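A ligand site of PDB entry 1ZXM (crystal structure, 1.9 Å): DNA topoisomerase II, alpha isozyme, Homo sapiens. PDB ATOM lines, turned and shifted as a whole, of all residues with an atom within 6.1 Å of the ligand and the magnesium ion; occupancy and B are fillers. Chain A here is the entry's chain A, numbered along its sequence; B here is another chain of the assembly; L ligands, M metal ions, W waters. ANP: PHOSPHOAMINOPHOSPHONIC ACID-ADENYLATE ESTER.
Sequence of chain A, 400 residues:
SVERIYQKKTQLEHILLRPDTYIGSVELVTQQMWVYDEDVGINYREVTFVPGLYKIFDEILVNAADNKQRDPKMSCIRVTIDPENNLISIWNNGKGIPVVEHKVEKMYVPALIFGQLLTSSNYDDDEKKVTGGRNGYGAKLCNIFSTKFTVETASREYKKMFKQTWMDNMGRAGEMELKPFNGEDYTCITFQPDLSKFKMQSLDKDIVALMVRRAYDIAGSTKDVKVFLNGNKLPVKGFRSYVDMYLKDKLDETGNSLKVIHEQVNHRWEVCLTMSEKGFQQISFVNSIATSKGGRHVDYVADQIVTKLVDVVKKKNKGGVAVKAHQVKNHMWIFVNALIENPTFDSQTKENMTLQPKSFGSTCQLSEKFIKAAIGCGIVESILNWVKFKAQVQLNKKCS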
ATOM      1  N   GLU A  59      -7.592  20.030  -7.785  1.00  0.00           N
ATOM      2  CA  GLU A  59      -6.564  19.193  -7.163  1.00  0.00           C
ATOM      3  C   GLU A  59      -7.131  18.353  -6.022  1.00  0.00           C
ATOM      4  O   GLU A  59      -6.799  17.163  -5.895  1.00  0.00           O
ATOM      5  CB  GLU A  59      -5.409  20.050  -6.645  1.00  0.00           C
ATOM      6  CG  GLU A  59      -4.600  20.765  -7.736  1.00  0.00           C
ATOM      7  CD  GLU A  59      -3.731  19.823  -8.556  1.00  0.00           C
ATOM      8  OE1 GLU A  59      -2.995  20.316  -9.442  1.00  0.00           O
ATOM      9  OE2 GLU A  59      -3.775  18.604  -8.335  1.00  0.00           O
ATOM     10  N   ILE A  60      -7.978  18.954  -5.202  1.00  0.00           N
ATOM     11  CA  ILE A  60      -8.545  18.237  -4.074  1.00  0.00           C
ATOM     12  C   ILE A  60      -9.576  17.207  -4.545  1.00  0.00           C
ATOM     13  O   ILE A  60      -9.647  16.104  -4.025  1.00  0.00           O
ATOM     14  CB  ILE A  60      -9.195  19.219  -3.068  1.00  0.00           C
ATOM     15  CG1 ILE A  60      -8.142  20.238  -2.601  1.00  0.00           C
ATOM     16  CG2 ILE A  60      -9.727  18.449  -1.859  1.00  0.00           C
ATOM     17  CD1 ILE A  60      -6.926  19.616  -1.947  1.00  0.00           C
ATOM     18  N   VAL A  62      -9.677  15.683  -7.506  1.00  0.00           N
ATOM     19  CA  VAL A  62      -9.004  14.552  -8.138  1.00  0.00           C
ATOM     20  C   VAL A  62      -8.389  13.645  -7.070  1.00  0.00           C
ATOM     21  O   VAL A  62      -8.357  12.431  -7.223  1.00  0.00           O
ATOM     22  CB  VAL A  62      -7.895  15.001  -9.122  1.00  0.00           C
ATOM     23  CG1 VAL A  62      -7.084  13.801  -9.579  1.00  0.00           C
ATOM     24  CG2 VAL A  62      -8.530  15.686 -10.338  1.00  0.00           C
ATOM     25  N   ASN A  63      -7.889  14.241  -5.991  1.00  0.00           N
ATOM     26  CA  ASN A  63      -7.319  13.440  -4.917  1.00  0.00           C
ATOM     27  C   ASN A  63      -8.380  12.516  -4.359  1.00  0.00           C
ATOM     28  O   ASN A  63      -8.094  11.355  -4.016  1.00  0.00           O
ATOM     29  CB  ASN A  63      -6.776  14.324  -3.784  1.00  0.00           C
ATOM     30  CG  ASN A  63      -5.419  14.923  -4.099  1.00  0.00           C
ATOM     31  OD1 ASN A  63      -4.729  14.471  -5.016  1.00  0.00           O
ATOM     32  ND2 ASN A  63      -5.011  15.924  -3.329  1.00  0.00           N
ATOM     33  N   ALA A  64      -9.609  13.005  -4.266  1.00  0.00           N
ATOM     34  CA  ALA A  64     -10.699  12.178  -3.740  1.00  0.00           C
ATOM     35  C   ALA A  64     -10.923  11.000  -4.689  1.00  0.00           C
ATOM     36  O   ALA A  64     -11.006   9.853  -4.251  1.00  0.00           O
ATOM     37  CB  ALA A  64     -11.968  12.999  -3.616  1.00  0.00           C
ATOM     38  N   ASP A  66      -8.840   9.698  -6.683  1.00  0.00           N
ATOM     39  CA  ASP A  66      -7.701   8.811  -6.607  1.00  0.00           C
ATOM     40  C   ASP A  66      -7.864   7.764  -5.500  1.00  0.00           C
ATOM     41  O   ASP A  66      -7.326   6.664  -5.616  1.00  0.00           O
ATOM     42  CB  ASP A  66      -6.392   9.576  -6.351  1.00  0.00           C
ATOM     43  CG  ASP A  66      -5.888  10.313  -7.582  1.00  0.00           C
ATOM     44  OD1 ASP A  66      -6.342   9.985  -8.702  1.00  0.00           O
ATOM     45  OD2 ASP A  66      -5.019  11.203  -7.438  1.00  0.00           O
ATOM     46  N   ASN A  67      -8.597   8.113  -4.443  1.00  0.00           N
ATOM     47  CA  ASN A  67      -8.774   7.163  -3.338  1.00  0.00           C
ATOM     48  C   ASN A  67      -9.645   5.970  -3.731  1.00  0.00           C
ATOM     49  O   ASN A  67      -9.578   4.925  -3.094  1.00  0.00           O
ATOM     50  CB  ASN A  67      -9.384   7.855  -2.095  1.00  0.00           C
ATOM     51  CG  ASN A  67      -9.072   7.094  -0.807  1.00  0.00           C
ATOM     52  OD1 ASN A  67      -7.920   6.800  -0.519  1.00  0.00           O
ATOM     53  ND2 ASN A  67     -10.107   6.779  -0.027  1.00  0.00           N
ATOM     54  N   ARG A  70      -7.215   3.549  -4.715  1.00  0.00           N
ATOM     55  CA  ARG A  70      -6.519   3.044  -3.533  1.00  0.00           C
ATOM     56  C   ARG A  70      -7.411   2.052  -2.781  1.00  0.00           C
ATOM     57  O   ARG A  70      -6.942   1.026  -2.304  1.00  0.00           O
ATOM     58  CB  ARG A  70      -6.125   4.220  -2.628  1.00  0.00           C
ATOM     59  CG  ARG A  70      -5.633   3.818  -1.237  1.00  0.00           C
ATOM     60  CD  ARG A  70      -4.912   4.978  -0.561  1.00  0.00           C
ATOM     61  NE  ARG A  70      -4.585   4.695   0.845  1.00  0.00           N
ATOM     62  CZ  ARG A  70      -5.354   5.037   1.870  1.00  0.00           C
ATOM     63  NH1 ARG A  70      -6.496   5.687   1.655  1.00  0.00           N
ATOM     64  NH2 ARG A  70      -4.981   4.737   3.112  1.00  0.00           N
ATOM     65  N   ASN A  92     -14.718  12.205   1.279  1.00  0.00           N
ATOM     66  CA  ASN A  92     -14.764  10.911   0.597  1.00  0.00           C
ATOM     67  C   ASN A  92     -14.659   9.789   1.615  1.00  0.00           C
ATOM     68  O   ASN A  92     -14.112   9.985   2.706  1.00  0.00           O
ATOM     69  CB  ASN A  92     -13.639  10.764  -0.447  1.00  0.00           C
ATOM     70  CG  ASN A  92     -12.261  10.638   0.169  1.00  0.00           C
ATOM     71  OD1 ASN A  92     -11.557  11.630   0.345  1.00  0.00           O
ATOM     72  ND2 ASN A  92     -11.869   9.413   0.502  1.00  0.00           N
ATOM     73  N   LYS A  95     -10.831   3.887   2.583  1.00  0.00           N
ATOM     74  CA  LYS A  95      -9.705   3.981   3.503  1.00  0.00           C
ATOM     75  C   LYS A  95      -9.199   5.400   3.759  1.00  0.00           C
ATOM     76  O   LYS A  95      -8.989   6.185   2.837  1.00  0.00           O
ATOM     77  CB  LYS A  95      -8.564   3.110   3.009  1.00  0.00           C
ATOM     78  N   GLY A  96      -9.003   5.713   5.035  1.00  0.00           N
ATOM     79  CA  GLY A  96      -8.504   7.016   5.406  1.00  0.00           C
ATOM     80  C   GLY A  96      -6.986   6.938   5.378  1.00  0.00           C
ATOM     81  O   GLY A  96      -6.431   5.862   5.166  1.00  0.00           O
ATOM     82  N   ILE A  97      -6.330   8.070   5.586  1.00  0.00           N
ATOM     83  CA  ILE A  97      -4.869   8.121   5.591  1.00  0.00           C
ATOM     84  C   ILE A  97      -4.324   7.601   6.920  1.00  0.00           C
ATOM     85  O   ILE A  97      -4.861   7.920   7.979  1.00  0.00           O
ATOM     86  CB  ILE A  97      -4.386   9.578   5.395  1.00  0.00           C
ATOM     87  CG1 ILE A  97      -4.925  10.121   4.060  1.00  0.00           C
ATOM     88  CG2 ILE A  97      -2.852   9.643   5.413  1.00  0.00           C
ATOM     89  CD1 ILE A  97      -4.718  11.606   3.878  1.00  0.00           C
ATOM     90  N   ILE A 113       2.159  14.922   4.156  1.00  0.00           N
ATOM     91  CA  ILE A 113       1.686  14.996   2.784  1.00  0.00           C
ATOM     92  C   ILE A 113       0.717  16.125   2.434  1.00  0.00           C
ATOM     93  O   ILE A 113       0.368  16.298   1.274  1.00  0.00           O
ATOM     94  CB  ILE A 113       1.064  13.647   2.353  1.00  0.00           C
ATOM     95  CG1 ILE A 113      -0.234  13.383   3.113  1.00  0.00           C
ATOM     96  CG2 ILE A 113       2.058  12.526   2.619  1.00  0.00           C
ATOM     97  CD1 ILE A 113      -0.864  12.028   2.757  1.00  0.00           C
ATOM     98  N   PHE A 114       0.291  16.899   3.431  1.00  0.00           N
ATOM     99  CA  PHE A 114      -0.585  18.041   3.181  1.00  0.00           C
ATOM    100  C   PHE A 114       0.101  19.331   3.591  1.00  0.00           C
ATOM    101  O   PHE A 114      -0.346  20.412   3.195  1.00  0.00           O
ATOM    102  CB  PHE A 114      -1.895  17.904   3.974  1.00  0.00           C
ATOM    103  CG  PHE A 114      -2.910  17.025   3.324  1.00  0.00           C
ATOM    104  CD1 PHE A 114      -3.668  17.490   2.257  1.00  0.00           C
ATOM    105  CD2 PHE A 114      -3.089  15.715   3.751  1.00  0.00           C
ATOM    106  CE1 PHE A 114      -4.595  16.667   1.618  1.00  0.00           C
ATOM    107  CE2 PHE A 114      -4.012  14.879   3.117  1.00  0.00           C
ATOM    108  CZ  PHE A 114      -4.765  15.359   2.040  1.00  0.00           C
ATOM    109  N   THR A 119       5.613  15.703  -1.577  1.00  0.00           N
ATOM    110  CA  THR A 119       5.297  14.528  -0.773  1.00  0.00           C
ATOM    111  C   THR A 119       4.175  13.811  -1.506  1.00  0.00           C
ATOM    112  O   THR A 119       3.195  14.426  -1.905  1.00  0.00           O
ATOM    113  CB  THR A 119       4.830  14.918   0.636  1.00  0.00           C
ATOM    114  OG1 THR A 119       3.839  15.947   0.536  1.00  0.00           O
ATOM    115  CG2 THR A 119       6.012  15.429   1.461  1.00  0.00           C
ATOM    116  N   SER A 120       4.306  12.500  -1.666  1.00  0.00           N
ATOM    117  CA  SER A 120       3.300  11.757  -2.399  1.00  0.00           C
ATOM    118  C   SER A 120       3.434  10.269  -2.161  1.00  0.00           C
ATOM    119  O   SER A 120       4.453   9.800  -1.642  1.00  0.00           O
ATOM    120  CB  SER A 120       3.483  12.054  -3.904  1.00  0.00           C
ATOM    121  OG  SER A 120       2.686  11.204  -4.719  1.00  0.00           O
ATOM    122  N   SER A 121       2.389   9.534  -2.534  1.00  0.00           N
ATOM    123  CA  SER A 121       2.414   8.082  -2.441  1.00  0.00           C
ATOM    124  C   SER A 121       2.527   7.585  -3.894  1.00  0.00           C
ATOM    125  O   SER A 121       2.454   6.387  -4.165  1.00  0.00           O
ATOM    126  CB  SER A 121       1.123   7.558  -1.785  1.00  0.00           C
ATOM    127  OG  SER A 121      -0.031   7.949  -2.513  1.00  0.00           O
ATOM    128  N   ASN A 122       2.725   8.523  -4.823  1.00  0.00           N
ATOM    129  CA  ASN A 122       2.808   8.196  -6.242  1.00  0.00           C
ATOM    130  C   ASN A 122       4.203   8.375  -6.871  1.00  0.00           C
ATOM    131  O   ASN A 122       4.315   8.589  -8.084  1.00  0.00           O
ATOM    132  CB  ASN A 122       1.800   9.039  -7.029  1.00  0.00           C
ATOM    133  CG  ASN A 122       0.349   8.675  -6.705  1.00  0.00           C
ATOM    134  OD1 ASN A 122      -0.100   7.580  -7.009  1.00  0.00           O
ATOM    135  ND2 ASN A 122      -0.385   9.603  -6.094  1.00  0.00           N
ATOM    136  N   GLY A 132      -4.532   9.801 -10.631  1.00  0.00           N
ATOM    137  CA  GLY A 132      -4.256  11.050 -11.313  1.00  0.00           C
ATOM    138  C   GLY A 132      -3.079  11.748 -10.653  1.00  0.00           C
ATOM    139  O   GLY A 132      -2.364  12.527 -11.297  1.00  0.00           O
ATOM    140  N   GLY A 133      -2.879  11.463  -9.371  1.00  0.00           N
ATOM    141  CA  GLY A 133      -1.793  12.080  -8.623  1.00  0.00           C
ATOM    142  C   GLY A 133      -0.439  11.641  -9.159  1.00  0.00           C
ATOM    143  O   GLY A 133      -0.247  10.461  -9.480  1.00  0.00           O
ATOM    144  N   ARG A 134       0.509  12.565  -9.236  1.00  0.00           N
ATOM    145  CA  ARG A 134       1.803  12.207  -9.781  1.00  0.00           C
ATOM    146  C   ARG A 134       3.021  12.960  -9.277  1.00  0.00           C
ATOM    147  O   ARG A 134       4.102  12.387  -9.120  1.00  0.00           O
ATOM    148  CB  ARG A 134       1.708  12.389 -11.290  1.00  0.00           C
ATOM    149  CG  ARG A 134       2.603  11.496 -12.045  1.00  0.00           C
ATOM    150  CD  ARG A 134       1.821  10.390 -12.715  1.00  0.00           C
ATOM    151  NE  ARG A 134       2.815   9.620 -13.439  1.00  0.00           N
ATOM    152  CZ  ARG A 134       3.571   8.707 -12.868  1.00  0.00           C
ATOM    153  NH1 ARG A 134       3.426   8.415 -11.585  1.00  0.00           N
ATOM    154  NH2 ARG A 134       4.532   8.127 -13.585  1.00  0.00           N
ATOM    155  N   ASN A 135       2.856  14.262  -9.030  1.00  0.00           N
ATOM    156  CA  ASN A 135       3.973  15.124  -8.635  1.00  0.00           C
ATOM    157  C   ASN A 135       4.181  15.435  -7.150  1.00  0.00           C
ATOM    158  O   ASN A 135       5.259  15.867  -6.768  1.00  0.00           O
ATOM    159  CB  ASN A 135       3.874  16.441  -9.401  1.00  0.00           C
ATOM    160  CG  ASN A 135       3.783  16.252 -10.913  1.00  0.00           C
ATOM    161  OD1 ASN A 135       3.206  17.090 -11.621  1.00  0.00           O
ATOM    162  ND2 ASN A 135       4.356  15.173 -11.411  1.00  0.00           N
ATOM    163  N   GLY A 136       3.152  15.270  -6.339  1.00  0.00           N
ATOM    164  CA  GLY A 136       3.296  15.575  -4.918  1.00  0.00           C
ATOM    165  C   GLY A 136       3.165  17.052  -4.598  1.00  0.00           C
ATOM    166  O   GLY A 136       3.753  17.542  -3.619  1.00  0.00           O
ATOM    167  N   TYR A 137       2.393  17.768  -5.417  1.00  0.00           N
ATOM    168  CA  TYR A 137       2.146  19.209  -5.276  1.00  0.00           C
ATOM    169  C   TYR A 137       0.698  19.606  -4.993  1.00  0.00           C
ATOM    170  O   TYR A 137       0.434  20.477  -4.166  1.00  0.00           O
ATOM    171  CB  TYR A 137       2.533  19.950  -6.563  1.00  0.00           C
ATOM    172  CG  TYR A 137       3.959  20.411  -6.656  1.00  0.00           C
ATOM    173  CD1 TYR A 137       4.854  19.793  -7.520  1.00  0.00           C
ATOM    174  CD2 TYR A 137       4.388  21.512  -5.930  1.00  0.00           C
ATOM    175  CE1 TYR A 137       6.155  20.267  -7.661  1.00  0.00           C
ATOM    176  CE2 TYR A 137       5.689  21.996  -6.068  1.00  0.00           C
ATOM    177  CZ  TYR A 137       6.562  21.369  -6.935  1.00  0.00           C
ATOM    178  OH  TYR A 137       7.841  21.853  -7.072  1.00  0.00           O
ATOM    179  N   GLY A 138      -0.223  18.994  -5.745  1.00  0.00           N
ATOM    180  CA  GLY A 138      -1.642  19.301  -5.657  1.00  0.00           C
ATOM    181  C   GLY A 138      -2.270  19.832  -4.382  1.00  0.00           C
ATOM    182  O   GLY A 138      -2.786  20.953  -4.354  1.00  0.00           O
ATOM    183  N   ALA A 139      -2.238  19.022  -3.335  1.00  0.00           N
ATOM    184  CA  ALA A 139      -2.840  19.408  -2.071  1.00  0.00           C
ATOM    185  C   ALA A 139      -2.132  20.596  -1.413  1.00  0.00           C
ATOM    186  O   ALA A 139      -2.779  21.455  -0.828  1.00  0.00           O
ATOM    187  CB  ALA A 139      -2.864  18.222  -1.128  1.00  0.00           C
ATOM    188  N   LYS A 140      -0.811  20.630  -1.520  1.00  0.00           N
ATOM    189  CA  LYS A 140      -0.067  21.734  -0.926  1.00  0.00           C
ATOM    190  C   LYS A 140      -0.364  23.019  -1.695  1.00  0.00           C
ATOM    191  O   LYS A 140      -0.350  24.104  -1.137  1.00  0.00           O
ATOM    192  CB  LYS A 140       1.439  21.434  -0.926  1.00  0.00           C
ATOM    193  CG  LYS A 140       1.905  20.553   0.233  1.00  0.00           C
ATOM    194  CD  LYS A 140       1.422  19.108   0.134  1.00  0.00           C
ATOM    195  CE  LYS A 140       2.130  18.368  -0.989  1.00  0.00           C
ATOM    196  NZ  LYS A 140       1.755  16.916  -1.053  1.00  0.00           N
ATOM    197  N   LEU A 141      -0.638  22.886  -2.991  1.00  0.00           N
ATOM    198  CA  LEU A 141      -0.944  24.063  -3.784  1.00  0.00           C
ATOM    199  C   LEU A 141      -2.261  24.672  -3.310  1.00  0.00           C
ATOM    200  O   LEU A 141      -2.373  25.881  -3.163  1.00  0.00           O
ATOM    201  CB  LEU A 141      -1.019  23.692  -5.267  1.00  0.00           C
ATOM    202  CG  LEU A 141       0.352  23.372  -5.898  1.00  0.00           C
ATOM    203  CD1 LEU A 141       0.162  22.933  -7.358  1.00  0.00           C
ATOM    204  CD2 LEU A 141       1.251  24.609  -5.804  1.00  0.00           C
ATOM    205  N   THR A 153      -8.943  13.241   8.661  1.00  0.00           N
ATOM    206  CA  THR A 153      -8.953  11.906   8.087  1.00  0.00           C
ATOM    207  C   THR A 153      -8.985  10.896   9.223  1.00  0.00           C
ATOM    208  O   THR A 153      -8.219  11.011  10.188  1.00  0.00           O
ATOM    209  CB  THR A 153      -7.703  11.680   7.186  1.00  0.00           C
ATOM    210  OG1 THR A 153      -7.820  10.437   6.489  1.00  0.00           O
ATOM    211  CG2 THR A 153      -6.425  11.671   8.020  1.00  0.00           C
ATOM    212  N   THR A 187     -12.144  10.959   4.704  1.00  0.00           N
ATOM    213  CA  THR A 187     -11.164  12.031   4.596  1.00  0.00           C
ATOM    214  C   THR A 187     -11.952  13.237   4.132  1.00  0.00           C
ATOM    215  O   THR A 187     -12.752  13.146   3.194  1.00  0.00           O
ATOM    216  CB  THR A 187     -10.045  11.703   3.581  1.00  0.00           C
ATOM    217  OG1 THR A 187      -9.228  10.647   4.100  1.00  0.00           O
ATOM    218  CG2 THR A 187      -9.168  12.940   3.328  1.00  0.00           C
ATOM    219  N   ILE A 189     -11.386  17.405   3.302  1.00  0.00           N
ATOM    220  CA  ILE A 189     -10.529  18.563   3.148  1.00  0.00           C
ATOM    221  C   ILE A 189     -11.441  19.777   3.054  1.00  0.00           C
ATOM    222  O   ILE A 189     -12.288  19.854   2.158  1.00  0.00           O
ATOM    223  CB  ILE A 189      -9.687  18.465   1.856  1.00  0.00           C
ATOM    224  CG1 ILE A 189      -8.888  17.153   1.853  1.00  0.00           C
ATOM    225  CG2 ILE A 189      -8.778  19.684   1.735  1.00  0.00           C
ATOM    226  CD1 ILE A 189      -7.957  16.959   3.029  1.00  0.00           C
ATOM    227  N   GLN A 348       1.834  20.905 -14.260  1.00  0.00           N
ATOM    228  CA  GLN A 348       1.115  20.489 -13.064  1.00  0.00           C
ATOM    229  C   GLN A 348      -0.394  20.559 -13.248  1.00  0.00           C
ATOM    230  O   GLN A 348      -1.135  19.801 -12.630  1.00  0.00           O
ATOM    231  CB  GLN A 348       1.546  21.381 -11.882  1.00  0.00           C
ATOM    232  CG  GLN A 348       0.790  21.130 -10.578  1.00  0.00           C
ATOM    233  CD  GLN A 348       0.984  19.726 -10.053  1.00  0.00           C
ATOM    234  OE1 GLN A 348       2.051  19.129 -10.209  1.00  0.00           O
ATOM    235  NE2 GLN A 348      -0.048  19.190  -9.397  1.00  0.00           N
ATOM    236  N   LYS A 350      -2.013  19.609 -15.676  1.00  0.00           N
ATOM    237  CA  LYS A 350      -2.407  18.383 -16.385  1.00  0.00           C
ATOM    238  C   LYS A 350      -3.526  18.519 -17.412  1.00  0.00           C
ATOM    239  O   LYS A 350      -4.457  17.705 -17.433  1.00  0.00           O
ATOM    240  CB  LYS A 350      -2.783  17.298 -15.382  1.00  0.00           C
ATOM    241  CG  LYS A 350      -1.777  17.100 -14.259  1.00  0.00           C
ATOM    242  CD  LYS A 350      -2.108  15.883 -13.428  1.00  0.00           C
ATOM    243  CE  LYS A 350      -1.468  15.946 -12.043  1.00  0.00           C
ATOM    244  NZ  LYS A 350      -0.020  16.261 -12.085  1.00  0.00           N
ATOM    245  N   TYR B   6       4.610   6.590   1.499  1.00  0.00           N
ATOM    246  CA  TYR B   6       4.618   8.053   1.547  1.00  0.00           C
ATOM    247  C   TYR B   6       6.053   8.573   1.556  1.00  0.00           C
ATOM    248  O   TYR B   6       6.782   8.428   2.536  1.00  0.00           O
ATOM    249  CB  TYR B   6       3.871   8.526   2.791  1.00  0.00           C
ATOM    250  CG  TYR B   6       2.430   8.069   2.786  1.00  0.00           C
ATOM    251  CD1 TYR B   6       1.504   8.633   1.907  1.00  0.00           C
ATOM    252  CD2 TYR B   6       2.016   7.020   3.608  1.00  0.00           C
ATOM    253  CE1 TYR B   6       0.196   8.167   1.851  1.00  0.00           C
ATOM    254  CE2 TYR B   6       0.712   6.542   3.557  1.00  0.00           C
ATOM    255  CZ  TYR B   6      -0.195   7.127   2.676  1.00  0.00           C
ATOM    256  OH  TYR B   6      -1.485   6.664   2.611  1.00  0.00           O
HETATM  257  PG  ANP L   1      -0.261  15.567  -7.620  1.00  0.00           P
HETATM  258  O1G ANP L   1      -1.679  15.908  -7.244  1.00  0.00           O
HETATM  259  O2G ANP L   1      -0.109  15.320  -9.177  1.00  0.00           O
HETATM  260  O3G ANP L   1       0.739  16.764  -7.283  1.00  0.00           O
HETATM  261  PB  ANP L   1      -0.381  13.772  -5.519  1.00  0.00           P
HETATM  262  O1B ANP L   1      -1.851  13.661  -5.650  1.00  0.00           O
HETATM  263  O2B ANP L   1       0.279  12.507  -5.081  1.00  0.00           O
HETATM  264  N3B ANP L   1       0.322  14.184  -6.935  1.00  0.00           N
HETATM  265  PA  ANP L   1      -0.727  15.636  -3.434  1.00  0.00           P
HETATM  266  O1A ANP L   1      -2.145  15.668  -3.789  1.00  0.00           O
HETATM  267  O2A ANP L   1      -0.122  16.959  -3.160  1.00  0.00           O
HETATM  268  O3A ANP L   1       0.127  14.990  -4.598  1.00  0.00           O
HETATM  269  O5' ANP L   1      -0.254  14.698  -2.206  1.00  0.00           O
HETATM  270  C5' ANP L   1      -1.172  14.347  -1.310  1.00  0.00           C
HETATM  271  C4' ANP L   1      -1.257  12.875  -1.033  1.00  0.00           C
HETATM  272  O4' ANP L   1      -2.375  12.818  -0.216  1.00  0.00           O
HETATM  273  C3' ANP L   1      -1.544  11.863  -2.136  1.00  0.00           C
HETATM  274  O3' ANP L   1      -0.311  11.439  -2.758  1.00  0.00           O
HETATM  275  C2' ANP L   1      -2.233  10.763  -1.319  1.00  0.00           C
HETATM  276  O2' ANP L   1      -1.328   9.714  -0.917  1.00  0.00           O
HETATM  277  C1' ANP L   1      -2.809  11.493  -0.067  1.00  0.00           C
HETATM  278  N9  ANP L   1      -4.294  11.778  -0.144  1.00  0.00           N
HETATM  279  C8  ANP L   1      -4.770  12.960  -0.640  1.00  0.00           C
HETATM  280  N7  ANP L   1      -6.079  13.022  -0.623  1.00  0.00           N
HETATM  281  C5  ANP L   1      -6.479  11.876  -0.122  1.00  0.00           C
HETATM  282  C6  ANP L   1      -7.743  11.380   0.135  1.00  0.00           C
HETATM  283  N6  ANP L   1      -8.815  12.115  -0.144  1.00  0.00           N
HETATM  284  N1  ANP L   1      -7.875  10.077   0.683  1.00  0.00           N
HETATM  285  C2  ANP L   1      -6.711   9.300   0.979  1.00  0.00           C
HETATM  286  N3  ANP L   1      -5.516   9.830   0.726  1.00  0.00           N
HETATM  287  C4  ANP L   1      -5.360  11.065   0.186  1.00  0.00           C
HETATM  288 MG    MG M   1      -3.097  15.235  -5.990  1.00  0.00          MG
HETATM  289  O   HOH W   1      -3.339   7.924   0.725  1.00  0.00           O
HETATM  290  O   HOH W   2      -2.478   6.592  -1.538  1.00  0.00           O
HETATM  291  O   HOH W   3      -6.839  15.966  -1.037  1.00  0.00           O
HETATM  292  O   HOH W   4      -3.977  14.094  -7.749  1.00  0.00           O
HETATM  293  O   HOH W   5      -4.213  16.849  -6.395  1.00  0.00           O
HETATM  294  O   HOH W   6      -5.540  10.708  -2.987  1.00  0.00           O
HETATM  295  O   HOH W   7      -9.443  14.967  -1.374  1.00  0.00           O
HETATM  296  O   HOH W   8      -3.758  11.390  -5.127  1.00  0.00           O
HETATM  297  O   HOH W   9      -9.480   8.964   2.261  1.00  0.00           O
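N of Tyr 137 lies within hydrogen-bond range of O3G of the ligand, at 2.7 Å.
The backbone NH (N) of Ser 121 sits at hydrogen-bond distance from an oxygen (O3') of the ligand (3.3 Å).
An oxygen (O2') of the ligand is in hydrogen-bond range of the side-chain hydroxyl of Ser 121, at 2.7 Å.
The side-chain hydroxyl (OG) of Ser 120 lies within hydrogen-bond range of an oxygen (O2B) of the ligand, at 2.8 Å.
An oxygen (O2G) of the ligand is in hydrogen-bond range of the backbone NH of Arg 134.
NZ of Lys 140 lies within salt-bridge range of O2A of the ligand, 2.8 Å away.
The side-chain amide oxygen of Asn 92 sits at hydrogen-bond distance from a nitrogen (N6) of the ligand, 2.8 Å away.
The backbone NH (N) of Gly 138 is in hydrogen-bond range of an oxygen (O3G) of the ligand.
The backbone NH (N) of Ala 139 sits at hydrogen-bond distance from an oxygen (O2A) of the ligand (3.0 Å).
N of Gly 136 is in hydrogen-bond range of O3G of the ligand (3.0 Å).
NZ of Lys 350 is in salt-bridge range of O2G of the ligand, 3.1 Å away.
ND2 of Asn 122 is in hydrogen-bond range of O2B of the ligand (3.1 Å).
O2G of the ligand sits at hydrogen-bond distance from N of Asn 135, 3.2 Å away.
A nitrogen (N1) of the ligand lies close to the side-chain amide oxygen of Asn 67, at 3.5 Å.
NE2 of Gln 348 sits at hydrogen-bond distance from O3G of the ligand (3.3 Å).
OG of Ser 120 lies within hydrogen-bond range of N of Asn 122 (2.7 Å).
NZ of Lys 140 sits at hydrogen-bond distance from O of Ile 113 (2.8 Å).
NZ of Lys 140 is in hydrogen-bond range of OG1 of Thr 119.
The side-chain amide nitrogen (ND2) of Asn 92 sits close to the side-chain amide nitrogen (ND2) of Asn 67, at 3.2 Å.
N of Asn 92 lies within hydrogen-bond range of O of Thr 187, at 2.9 Å.
The side-chain amide nitrogen of Asn 122 lies close to the backbone carbonyl oxygen of Gly 133 (3.5 Å).
The side-chain amide oxygen (OD1) of Asn 135 sits close to the side-chain amide oxygen (OE1) of Gln 348, 2.7 Å away.
The backbone NH (N) of Gly 133 sits at hydrogen-bond distance from the side-chain carboxylate (OD2) of Asp 66, at 2.9 Å.
An oxygen (O5') of the ligand lies close to the backbone carbonyl oxygen (O) of Thr 119, 3.5 Å away.
Glu 59 touches the ligand (OE2 to O1G, 3.6 Å).
Arg 70 touches the ligand (NH1 to C2, 3.7 Å).
Ile 97 touches the ligand.
Ile 113 touches the ligand.
Phe 114 touches the ligand.
Gly 133 touches the ligand (CA to O1B, 3.4 Å).
CG2 of Thr 187 touches N6 of the ligand, 3.6 Å away.
Tyr 6 of chain B touches the ligand.
Hydrophobic or aromatic side chains within 4 Å of the ligand: Ile 97, Ile 113, Phe 114, Tyr 137, Ala 139 and Tyr 6 of chain B.
Of the 34 residues printed, 24 come within 4 Å of the ligand.
The nearest printed residue that does not touch the ligand is Ala 64 (4.1 Å).
The magnesium ion is bound by water W5 (2.0 Å), an oxygen (O1G) of the ligand (2.0 Å), an oxygen (O1B) of the ligand (2.0 Å), the side-chain amide oxygen (OD1) of Asn 63 (2.0 Å), water W4 (2.3 Å) and an oxygen (O1A) of the ligand (2.4 Å).
Water W4 bridges the side-chain carboxylate (OD2) of Asp 66 (3.1 Å) and the backbone NH (N) of Gly 133 (3.3 Å).
Water W5 bridges OE2 of Glu 59 (2.7 Å) and ND2 of Asn 63 (3.3 Å).
Water W9 lies within hydrogen-bond range of the side-chain hydroxyl (OG1) of Thr 187 (2.5 Å), a nitrogen (N1) of the ligand (2.5 Å), the backbone carbonyl oxygen (O) of Lys 95 (2.9 Å), the side-chain amide nitrogen (ND2) of Asn 92 (3.0 Å) and the side-chain amide nitrogen (ND2) of Asn 67 (3.2 Å).
Water W1 lies within hydrogen-bond range of a nitrogen (N3) of the ligand (2.9 Å), the side-chain hydroxyl of Tyr 6 of chain B (2.9 Å) and the guanidinium group of Arg 70 (3.5 Å).
Water W3 bridges ND2 of Asn 63 and N7 of the ligand.
Water W2 lies within hydrogen-bond range of OG of Ser 121 and O2' of the ligand.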
